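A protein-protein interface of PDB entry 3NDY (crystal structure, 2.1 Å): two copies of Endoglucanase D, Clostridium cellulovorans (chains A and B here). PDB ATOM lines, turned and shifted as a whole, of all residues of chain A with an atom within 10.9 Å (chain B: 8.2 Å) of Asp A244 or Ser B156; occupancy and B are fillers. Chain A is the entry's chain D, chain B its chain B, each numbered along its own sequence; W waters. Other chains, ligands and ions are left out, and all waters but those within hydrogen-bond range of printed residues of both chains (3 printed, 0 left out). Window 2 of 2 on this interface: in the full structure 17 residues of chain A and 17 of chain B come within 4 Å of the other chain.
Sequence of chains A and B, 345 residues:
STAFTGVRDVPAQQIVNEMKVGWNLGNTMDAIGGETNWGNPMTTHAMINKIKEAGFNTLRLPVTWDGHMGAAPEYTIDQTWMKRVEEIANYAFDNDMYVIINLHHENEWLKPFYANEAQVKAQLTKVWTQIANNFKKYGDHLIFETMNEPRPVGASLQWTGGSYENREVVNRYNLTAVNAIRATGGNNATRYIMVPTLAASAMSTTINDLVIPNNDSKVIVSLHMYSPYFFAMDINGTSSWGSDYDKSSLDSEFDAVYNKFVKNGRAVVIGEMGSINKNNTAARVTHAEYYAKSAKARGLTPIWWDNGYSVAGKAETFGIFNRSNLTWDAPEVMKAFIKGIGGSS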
ATOM      1  N   PRO A 228      28.096 -27.090  15.000  1.00  0.00           N
ATOM      2  CA  PRO A 228      29.517 -26.847  14.748  1.00  0.00           C
ATOM      3  C   PRO A 228      30.055 -27.979  13.896  1.00  0.00           C
ATOM      4  O   PRO A 228      29.553 -29.105  13.988  1.00  0.00           O
ATOM      5  CB  PRO A 228      30.132 -26.898  16.150  1.00  0.00           C
ATOM      6  CG  PRO A 228      29.263 -27.841  16.895  1.00  0.00           C
ATOM      7  CD  PRO A 228      27.870 -27.743  16.303  1.00  0.00           C
ATOM      8  N   SER A 240      29.663 -35.702  21.121  1.00  0.00           N
ATOM      9  CA  SER A 240      28.999 -35.007  22.217  1.00  0.00           C
ATOM     10  C   SER A 240      28.761 -33.537  21.917  1.00  0.00           C
ATOM     11  O   SER A 240      29.589 -32.886  21.282  1.00  0.00           O
ATOM     12  CB  SER A 240      29.823 -35.135  23.501  1.00  0.00           C
ATOM     13  OG  SER A 240      29.723 -36.447  24.026  1.00  0.00           O
ATOM     14  N   TRP A 241      27.626 -33.022  22.384  1.00  0.00           N
ATOM     15  CA  TRP A 241      27.308 -31.608  22.248  1.00  0.00           C
ATOM     16  C   TRP A 241      26.442 -31.195  23.420  1.00  0.00           C
ATOM     17  O   TRP A 241      25.469 -31.877  23.739  1.00  0.00           O
ATOM     18  CB  TRP A 241      26.556 -31.323  20.938  1.00  0.00           C
ATOM     19  CG  TRP A 241      26.523 -29.862  20.622  1.00  0.00           C
ATOM     20  CD1 TRP A 241      27.395 -29.181  19.818  1.00  0.00           C
ATOM     21  CD2 TRP A 241      25.605 -28.883  21.139  1.00  0.00           C
ATOM     22  NE1 TRP A 241      27.070 -27.843  19.795  1.00  0.00           N
ATOM     23  CE2 TRP A 241      25.974 -27.636  20.591  1.00  0.00           C
ATOM     24  CE3 TRP A 241      24.498 -28.944  21.995  1.00  0.00           C
ATOM     25  CZ2 TRP A 241      25.282 -26.457  20.880  1.00  0.00           C
ATOM     26  CZ3 TRP A 241      23.815 -27.773  22.282  1.00  0.00           C
ATOM     27  CH2 TRP A 241      24.214 -26.544  21.727  1.00  0.00           C
ATOM     28  N   GLY A 242      26.785 -30.081  24.065  1.00  0.00           N
ATOM     29  CA  GLY A 242      25.966 -29.589  25.159  1.00  0.00           C
ATOM     30  C   GLY A 242      26.640 -28.676  26.168  1.00  0.00           C
ATOM     31  O   GLY A 242      25.966 -28.065  26.998  1.00  0.00           O
ATOM     32  N   SER A 243      27.960 -28.567  26.102  1.00  0.00           N
ATOM     33  CA  SER A 243      28.694 -27.738  27.054  1.00  0.00           C
ATOM     34  C   SER A 243      28.357 -26.252  26.890  1.00  0.00           C
ATOM     35  O   SER A 243      27.778 -25.843  25.882  1.00  0.00           O
ATOM     36  CB  SER A 243      30.194 -27.936  26.884  1.00  0.00           C
ATOM     37  OG  SER A 243      30.633 -27.313  25.689  1.00  0.00           O
ATOM     38  N   ASP A 244      28.713 -25.452  27.891  1.00  0.00           N
ATOM     39  CA  ASP A 244      28.511 -24.014  27.813  1.00  0.00           C
ATOM     40  C   ASP A 244      29.318 -23.471  26.651  1.00  0.00           C
ATOM     41  O   ASP A 244      28.899 -22.538  25.971  1.00  0.00           O
ATOM     42  CB  ASP A 244      28.946 -23.332  29.108  1.00  0.00           C
ATOM     43  CG  ASP A 244      27.967 -23.566  30.243  1.00  0.00           C
ATOM     44  OD1 ASP A 244      26.786 -23.856  29.957  1.00  0.00           O
ATOM     45  OD2 ASP A 244      28.377 -23.456  31.415  1.00  0.00           O
ATOM     46  N   TYR A 245      30.479 -24.065  26.419  1.00  0.00           N
ATOM     47  CA  TYR A 245      31.293 -23.651  25.293  1.00  0.00           C
ATOM     48  C   TYR A 245      30.569 -23.913  23.970  1.00  0.00           C
ATOM     49  O   TYR A 245      30.569 -23.067  23.083  1.00  0.00           O
ATOM     50  CB  TYR A 245      32.635 -24.366  25.293  1.00  0.00           C
ATOM     51  CG  TYR A 245      33.382 -24.142  24.013  1.00  0.00           C
ATOM     52  CD1 TYR A 245      34.107 -22.975  23.811  1.00  0.00           C
ATOM     53  CD2 TYR A 245      33.349 -25.088  22.988  1.00  0.00           C
ATOM     54  CE1 TYR A 245      34.794 -22.755  22.630  1.00  0.00           C
ATOM     55  CE2 TYR A 245      34.037 -24.872  21.795  1.00  0.00           C
ATOM     56  CZ  TYR A 245      34.755 -23.704  21.625  1.00  0.00           C
ATOM     57  OH  TYR A 245      35.442 -23.472  20.452  1.00  0.00           O
ATOM     58  N   ASP A 246      29.952 -25.087  23.847  1.00  0.00           N
ATOM     59  CA  ASP A 246      29.227 -25.447  22.632  1.00  0.00           C
ATOM     60  C   ASP A 246      28.109 -24.438  22.391  1.00  0.00           C
ATOM     61  O   ASP A 246      27.942 -23.937  21.287  1.00  0.00           O
ATOM     62  CB  ASP A 246      28.612 -26.847  22.753  1.00  0.00           C
ATOM     63  CG  ASP A 246      29.646 -27.961  22.748  1.00  0.00           C
ATOM     64  OD1 ASP A 246      30.735 -27.794  22.165  1.00  0.00           O
ATOM     65  OD2 ASP A 246      29.352 -29.021  23.329  1.00  0.00           O
ATOM     66  N   LYS A 247      27.345 -24.154  23.439  1.00  0.00           N
ATOM     67  CA  LYS A 247      26.220 -23.234  23.341  1.00  0.00           C
ATOM     68  C   LYS A 247      26.679 -21.835  22.966  1.00  0.00           C
ATOM     69  O   LYS A 247      26.056 -21.171  22.134  1.00  0.00           O
ATOM     70  CB  LYS A 247      25.443 -23.195  24.655  1.00  0.00           C
ATOM     71  CG  LYS A 247      24.767 -24.519  24.990  1.00  0.00           C
ATOM     72  CD  LYS A 247      23.924 -24.408  26.244  1.00  0.00           C
ATOM     73  CE  LYS A 247      23.305 -25.744  26.613  1.00  0.00           C
ATOM     74  NZ  LYS A 247      22.483 -25.632  27.853  1.00  0.00           N
ATOM     75  N   SER A 248      27.771 -21.394  23.584  1.00  0.00           N
ATOM     76  CA  SER A 248      28.312 -20.063  23.326  1.00  0.00           C
ATOM     77  C   SER A 248      28.828 -19.921  21.887  1.00  0.00           C
ATOM     78  O   SER A 248      28.576 -18.914  21.220  1.00  0.00           O
ATOM     79  CB  SER A 248      29.415 -19.734  24.335  1.00  0.00           C
ATOM     80  OG  SER A 248      30.178 -18.623  23.909  1.00  0.00           O
ATOM     81  N   SER A 249      29.530 -20.939  21.403  1.00  0.00           N
ATOM     82  CA  SER A 249      30.093 -20.897  20.055  1.00  0.00           C
ATOM     83  C   SER A 249      28.999 -20.838  19.002  1.00  0.00           C
ATOM     84  O   SER A 249      29.089 -20.079  18.044  1.00  0.00           O
ATOM     85  CB  SER A 249      30.981 -22.116  19.794  1.00  0.00           C
ATOM     86  OG  SER A 249      31.994 -22.212  20.779  1.00  0.00           O
ATOM     87  N   LEU A 250      27.971 -21.658  19.174  1.00  0.00           N
ATOM     88  CA  LEU A 250      26.870 -21.674  18.230  1.00  0.00           C
ATOM     89  C   LEU A 250      26.149 -20.319  18.198  1.00  0.00           C
ATOM     90  O   LEU A 250      25.818 -19.803  17.121  1.00  0.00           O
ATOM     91  CB  LEU A 250      25.895 -22.794  18.579  1.00  0.00           C
ATOM     92  CG  LEU A 250      24.867 -23.069  17.483  1.00  0.00           C
ATOM     93  CD1 LEU A 250      25.578 -23.486  16.208  1.00  0.00           C
ATOM     94  CD2 LEU A 250      23.878 -24.130  17.921  1.00  0.00           C
ATOM     95  N   ASP A 251      25.908 -19.753  19.380  1.00  0.00           N
ATOM     96  CA  ASP A 251      25.277 -18.443  19.495  1.00  0.00           C
ATOM     97  C   ASP A 251      26.086 -17.437  18.692  1.00  0.00           C
ATOM     98  O   ASP A 251      25.529 -16.602  17.982  1.00  0.00           O
ATOM     99  CB  ASP A 251      25.261 -17.962  20.948  1.00  0.00           C
ATOM    100  CG  ASP A 251      24.219 -18.657  21.798  1.00  0.00           C
ATOM    101  OD1 ASP A 251      23.385 -19.406  21.261  1.00  0.00           O
ATOM    102  OD2 ASP A 251      24.240 -18.443  23.023  1.00  0.00           O
ATOM    103  N   SER A 252      27.406 -17.507  18.834  1.00  0.00           N
ATOM    104  CA  SER A 252      28.280 -16.510  18.222  1.00  0.00           C
ATOM    105  C   SER A 252      28.258 -16.618  16.706  1.00  0.00           C
ATOM    106  O   SER A 252      28.330 -15.610  16.001  1.00  0.00           O
ATOM    107  CB  SER A 252      29.708 -16.646  18.752  1.00  0.00           C
ATOM    108  OG  SER A 252      30.514 -15.591  18.284  1.00  0.00           O
ATOM    109  N   GLU A 253      28.164 -17.843  16.198  1.00  0.00           N
ATOM    110  CA  GLU A 253      28.002 -18.038  14.763  1.00  0.00           C
ATOM    111  C   GLU A 253      26.741 -17.343  14.261  1.00  0.00           C
ATOM    112  O   GLU A 253      26.774 -16.661  13.243  1.00  0.00           O
ATOM    113  CB  GLU A 253      27.979 -19.529  14.395  1.00  0.00           C
ATOM    114  CG  GLU A 253      29.344 -20.197  14.510  1.00  0.00           C
ATOM    115  CD  GLU A 253      29.361 -21.606  13.930  1.00  0.00           C
ATOM    116  OE1 GLU A 253      29.118 -21.764  12.710  1.00  0.00           O
ATOM    117  OE2 GLU A 253      29.628 -22.556  14.699  1.00  0.00           O
ATOM    118  N   THR A 286      19.813 -32.615  22.035  1.00  0.00           N
ATOM    119  CA  THR A 286      20.277 -31.399  22.696  1.00  0.00           C
ATOM    120  C   THR A 286      20.696 -30.344  21.676  1.00  0.00           C
ATOM    121  O   THR A 286      20.235 -29.200  21.736  1.00  0.00           O
ATOM    122  CB  THR A 286      21.461 -31.697  23.647  1.00  0.00           C
ATOM    123  OG1 THR A 286      21.061 -32.694  24.594  1.00  0.00           O
ATOM    124  CG2 THR A 286      21.897 -30.437  24.394  1.00  0.00           C
ATOM    125  N   TYR A 290      18.611 -26.793  20.714  1.00  0.00           N
ATOM    126  CA  TYR A 290      19.324 -25.544  20.961  1.00  0.00           C
ATOM    127  C   TYR A 290      19.549 -24.750  19.653  1.00  0.00           C
ATOM    128  O   TYR A 290      19.325 -23.540  19.603  1.00  0.00           O
ATOM    129  CB  TYR A 290      20.657 -25.783  21.680  1.00  0.00           C
ATOM    130  CG  TYR A 290      21.224 -24.492  22.210  1.00  0.00           C
ATOM    131  CD1 TYR A 290      20.883 -24.028  23.479  1.00  0.00           C
ATOM    132  CD2 TYR A 290      22.044 -23.701  21.422  1.00  0.00           C
ATOM    133  CE1 TYR A 290      21.378 -22.818  23.956  1.00  0.00           C
ATOM    134  CE2 TYR A 290      22.544 -22.502  21.884  1.00  0.00           C
ATOM    135  CZ  TYR A 290      22.208 -22.058  23.148  1.00  0.00           C
ATOM    136  OH  TYR A 290      22.707 -20.860  23.602  1.00  0.00           O
ATOM    137  N   SER A 294      18.201 -20.983  19.198  1.00  0.00           N
ATOM    138  CA  SER A 294      19.253 -19.968  19.098  1.00  0.00           C
ATOM    139  C   SER A 294      19.188 -19.262  17.741  1.00  0.00           C
ATOM    140  O   SER A 294      19.328 -18.040  17.654  1.00  0.00           O
ATOM    141  CB  SER A 294      20.635 -20.591  19.317  1.00  0.00           C
ATOM    142  OG  SER A 294      21.673 -19.623  19.211  1.00  0.00           O
ATOM    143  N   PRO B 152      33.661 -13.850  33.275  1.00  0.00           N
ATOM    144  CA  PRO B 152      33.198 -14.606  34.450  1.00  0.00           C
ATOM    145  C   PRO B 152      34.172 -15.749  34.759  1.00  0.00           C
ATOM    146  O   PRO B 152      34.610 -16.413  33.825  1.00  0.00           O
ATOM    147  CB  PRO B 152      31.858 -15.174  33.982  1.00  0.00           C
ATOM    148  CG  PRO B 152      32.048 -15.350  32.485  1.00  0.00           C
ATOM    149  CD  PRO B 152      32.857 -14.136  32.073  1.00  0.00           C
ATOM    150  N   VAL B 153      34.527 -15.961  36.026  1.00  0.00           N
ATOM    151  CA  VAL B 153      35.436 -17.057  36.387  1.00  0.00           C
ATOM    152  C   VAL B 153      34.801 -18.423  36.143  1.00  0.00           C
ATOM    153  O   VAL B 153      33.580 -18.565  36.169  1.00  0.00           O
ATOM    154  CB  VAL B 153      35.875 -17.001  37.876  1.00  0.00           C
ATOM    155  CG1 VAL B 153      36.763 -15.799  38.135  1.00  0.00           C
ATOM    156  CG2 VAL B 153      34.663 -16.983  38.790  1.00  0.00           C
ATOM    157  N   GLY B 154      35.635 -19.433  35.930  1.00  0.00           N
ATOM    158  CA  GLY B 154      35.144 -20.781  35.685  1.00  0.00           C
ATOM    159  C   GLY B 154      35.842 -21.400  34.489  1.00  0.00           C
ATOM    160  O   GLY B 154      35.868 -20.820  33.401  1.00  0.00           O
ATOM    161  N   ALA B 155      36.425 -22.576  34.691  1.00  0.00           N
ATOM    162  CA  ALA B 155      37.146 -23.250  33.619  1.00  0.00           C
ATOM    163  C   ALA B 155      36.268 -23.397  32.377  1.00  0.00           C
ATOM    164  O   ALA B 155      36.726 -23.185  31.250  1.00  0.00           O
ATOM    165  CB  ALA B 155      37.642 -24.614  34.087  1.00  0.00           C
ATOM    166  N   SER B 156      35.005 -23.753  32.601  1.00  0.00           N
ATOM    167  CA  SER B 156      34.078 -24.074  31.524  1.00  0.00           C
ATOM    168  C   SER B 156      33.632 -22.846  30.729  1.00  0.00           C
ATOM    169  O   SER B 156      32.975 -22.985  29.692  1.00  0.00           O
ATOM    170  CB  SER B 156      32.859 -24.823  32.077  1.00  0.00           C
ATOM    171  OG  SER B 156      31.875 -23.936  32.581  1.00  0.00           O
ATOM    172  N   LEU B 157      33.990 -21.656  31.210  1.00  0.00           N
ATOM    173  CA  LEU B 157      33.555 -20.414  30.574  1.00  0.00           C
ATOM    174  C   LEU B 157      34.702 -19.714  29.869  1.00  0.00           C
ATOM    175  O   LEU B 157      34.506 -18.679  29.236  1.00  0.00           O
ATOM    176  CB  LEU B 157      32.937 -19.462  31.602  1.00  0.00           C
ATOM    177  CG  LEU B 157      31.732 -19.994  32.373  1.00  0.00           C
ATOM    178  CD1 LEU B 157      31.282 -18.985  33.432  1.00  0.00           C
ATOM    179  CD2 LEU B 157      30.594 -20.344  31.415  1.00  0.00           C
ATOM    180  N   GLN B 158      35.896 -20.286  29.977  1.00  0.00           N
ATOM    181  CA  GLN B 158      37.123 -19.660  29.484  1.00  0.00           C
ATOM    182  C   GLN B 158      37.053 -19.129  28.041  1.00  0.00           C
ATOM    183  O   GLN B 158      37.537 -18.033  27.741  1.00  0.00           O
ATOM    184  CB  GLN B 158      38.294 -20.641  29.645  1.00  0.00           C
ATOM    185  CG  GLN B 158      39.396 -20.496  28.604  1.00  0.00           C
ATOM    186  CD  GLN B 158      40.646 -19.816  29.139  1.00  0.00           C
ATOM    187  OE1 GLN B 158      41.770 -20.183  28.780  1.00  0.00           O
ATOM    188  NE2 GLN B 158      40.457 -18.820  30.000  1.00  0.00           N
ATOM    189  N   TRP B 159      36.455 -19.911  27.151  1.00  0.00           N
ATOM    190  CA  TRP B 159      36.390 -19.547  25.744  1.00  0.00           C
ATOM    191  C   TRP B 159      34.967 -19.236  25.307  1.00  0.00           C
ATOM    192  O   TRP B 159      34.611 -19.452  24.149  1.00  0.00           O
ATOM    193  CB  TRP B 159      36.955 -20.672  24.874  1.00  0.00           C
ATOM    194  CG  TRP B 159      38.383 -20.993  25.171  1.00  0.00           C
ATOM    195  CD1 TRP B 159      38.859 -22.071  25.864  1.00  0.00           C
ATOM    196  CD2 TRP B 159      39.529 -20.221  24.793  1.00  0.00           C
ATOM    197  NE1 TRP B 159      40.232 -22.020  25.933  1.00  0.00           N
ATOM    198  CE2 TRP B 159      40.667 -20.893  25.285  1.00  0.00           C
ATOM    199  CE3 TRP B 159      39.702 -19.026  24.086  1.00  0.00           C
ATOM    200  CZ2 TRP B 159      41.959 -20.409  25.093  1.00  0.00           C
ATOM    201  CZ3 TRP B 159      40.987 -18.549  23.895  1.00  0.00           C
ATOM    202  CH2 TRP B 159      42.098 -19.239  24.397  1.00  0.00           C
ATOM    203  N   THR B 160      34.148 -18.759  26.238  1.00  0.00           N
ATOM    204  CA  THR B 160      32.789 -18.358  25.904  1.00  0.00           C
ATOM    205  C   THR B 160      32.724 -16.846  25.819  1.00  0.00           C
ATOM    206  O   THR B 160      33.700 -16.161  26.140  1.00  0.00           O
ATOM    207  CB  THR B 160      31.762 -18.870  26.930  1.00  0.00           C
ATOM    208  OG1 THR B 160      31.929 -18.183  28.180  1.00  0.00           O
ATOM    209  CG2 THR B 160      31.920 -20.380  27.142  1.00  0.00           C
ATOM    210  N   GLY B 161      31.584 -16.326  25.374  1.00  0.00           N
ATOM    211  CA  GLY B 161      31.377 -14.891  25.309  1.00  0.00           C
ATOM    212  C   GLY B 161      30.608 -14.360  26.514  1.00  0.00           C
ATOM    213  O   GLY B 161      30.115 -13.239  26.500  1.00  0.00           O
ATOM    214  N   GLY B 162      30.496 -15.172  27.558  1.00  0.00           N
ATOM    215  CA  GLY B 162      29.817 -14.753  28.770  1.00  0.00           C
ATOM    216  C   GLY B 162      28.313 -14.671  28.592  1.00  0.00           C
ATOM    217  O   GLY B 162      27.776 -15.098  27.578  1.00  0.00           O
HETATM  218  O   HOH W   1      32.367 -19.654  22.531  1.00  0.00           O
HETATM  219  O   HOH W   2      32.180 -25.255  28.463  1.00  0.00           O
HETATM  220  O   HOH W   3      28.515 -16.602  25.478  1.00  0.00           O
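OG of Ser A248 sits at hydrogen-bond distance from N of Gly B161.
OG of Ser A243 sits close to N of Tyr A245, 3.3 Å away. N of Gly B162 sits close to OG1 of Thr B160 (3.4 Å). O of Leu B157 sits at hydrogen-bond distance from OG1 of Thr B160, 2.8 Å away. OG of Ser A249 is in hydrogen-bond range of O of Tyr A245 (2.8 Å).
Among the printed residues, pairs that only touch across the chains: Asp A244 with Ser B156 (3.7 Å), Asp A244 with Leu B157 (3.8 Å), Asp A244 with Thr B160 (3.9 Å), Tyr A245 with Trp B159 (3.6 Å), Tyr A245 with Thr B160 (3.8 Å) and Ser A248 with Thr B160 (3.3 Å).
Asp A244 touches just these residues of chain B: Ser B156 (3.7 Å), Leu B157 (3.8 Å) and Thr B160 (3.9 Å). Ser B156 touches just one residue of chain A: Asp A244 (3.7 Å). No residue of chain B comes within 4 Å of Ser A243. No residue of chain A comes within 4 Å of Gly B154. No residue of chain A comes within 4 Å of Ala B155. Printed residues of chain A within 4 Å of Leu B157: Asp A244 (3.8 Å). Printed residues of chain B within 4 Å of Tyr A245: Trp B159 and Thr B160. Of the printed residues of chain A, Gly B161 touches Ser A248 (3.1 Å). Of the printed residues of chain A, Thr B160 touches Asp A244, Tyr A245 and Ser A248. Of the printed residues of chain A, Trp B159 touches Tyr A245 (3.6 Å). Gln B158 touches none of the printed residues of chain A. Val B153 touches none of the printed residues of chain A. The nearest residue of chain A that does not touch Ser B156 is Tyr A245 (4.3 Å). The nearest printed residue of chain B that does not touch Ser A248 is Trp B159 (4.5 Å).
Printed residues of chain A that touch a printed residue of chain B: Asp A244, Tyr A245 and Ser A248. Hydrophobic or aromatic side chains of chain A that line the printed part of chain B: Tyr A245. Of the 11 printed residues of chain B, 5 touch a printed residue of chain A. Printed residues of chain B that touch a printed residue of chain A: Ser B156, Leu B157, Trp B159, Thr B160 and Gly B161. Hydrophobic or aromatic side chains of chain B within 4 Å of the printed part of chain A: Leu B157 and Trp B159. Among the printed residues, no Asp or Glu carboxylate lies within 4 Å of a Lys or Arg side-chain nitrogen of the other chain.
No position is printed for both chains.
Water W3 lies within hydrogen-bond range of the backbone carbonyl oxygen of Gly B162 (2.7 Å), the side-chain hydroxyl of Ser A248 (3.1 Å) and the backbone NH of Gly B161 (3.1 Å). Water W2 lies within hydrogen-bond range of O of Ser B156 (2.7 Å) and N of Tyr A245 (2.9 Å). Water W1 lies within hydrogen-bond range of O of Trp B159, OG of Ser A248 and OG of Ser A249.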
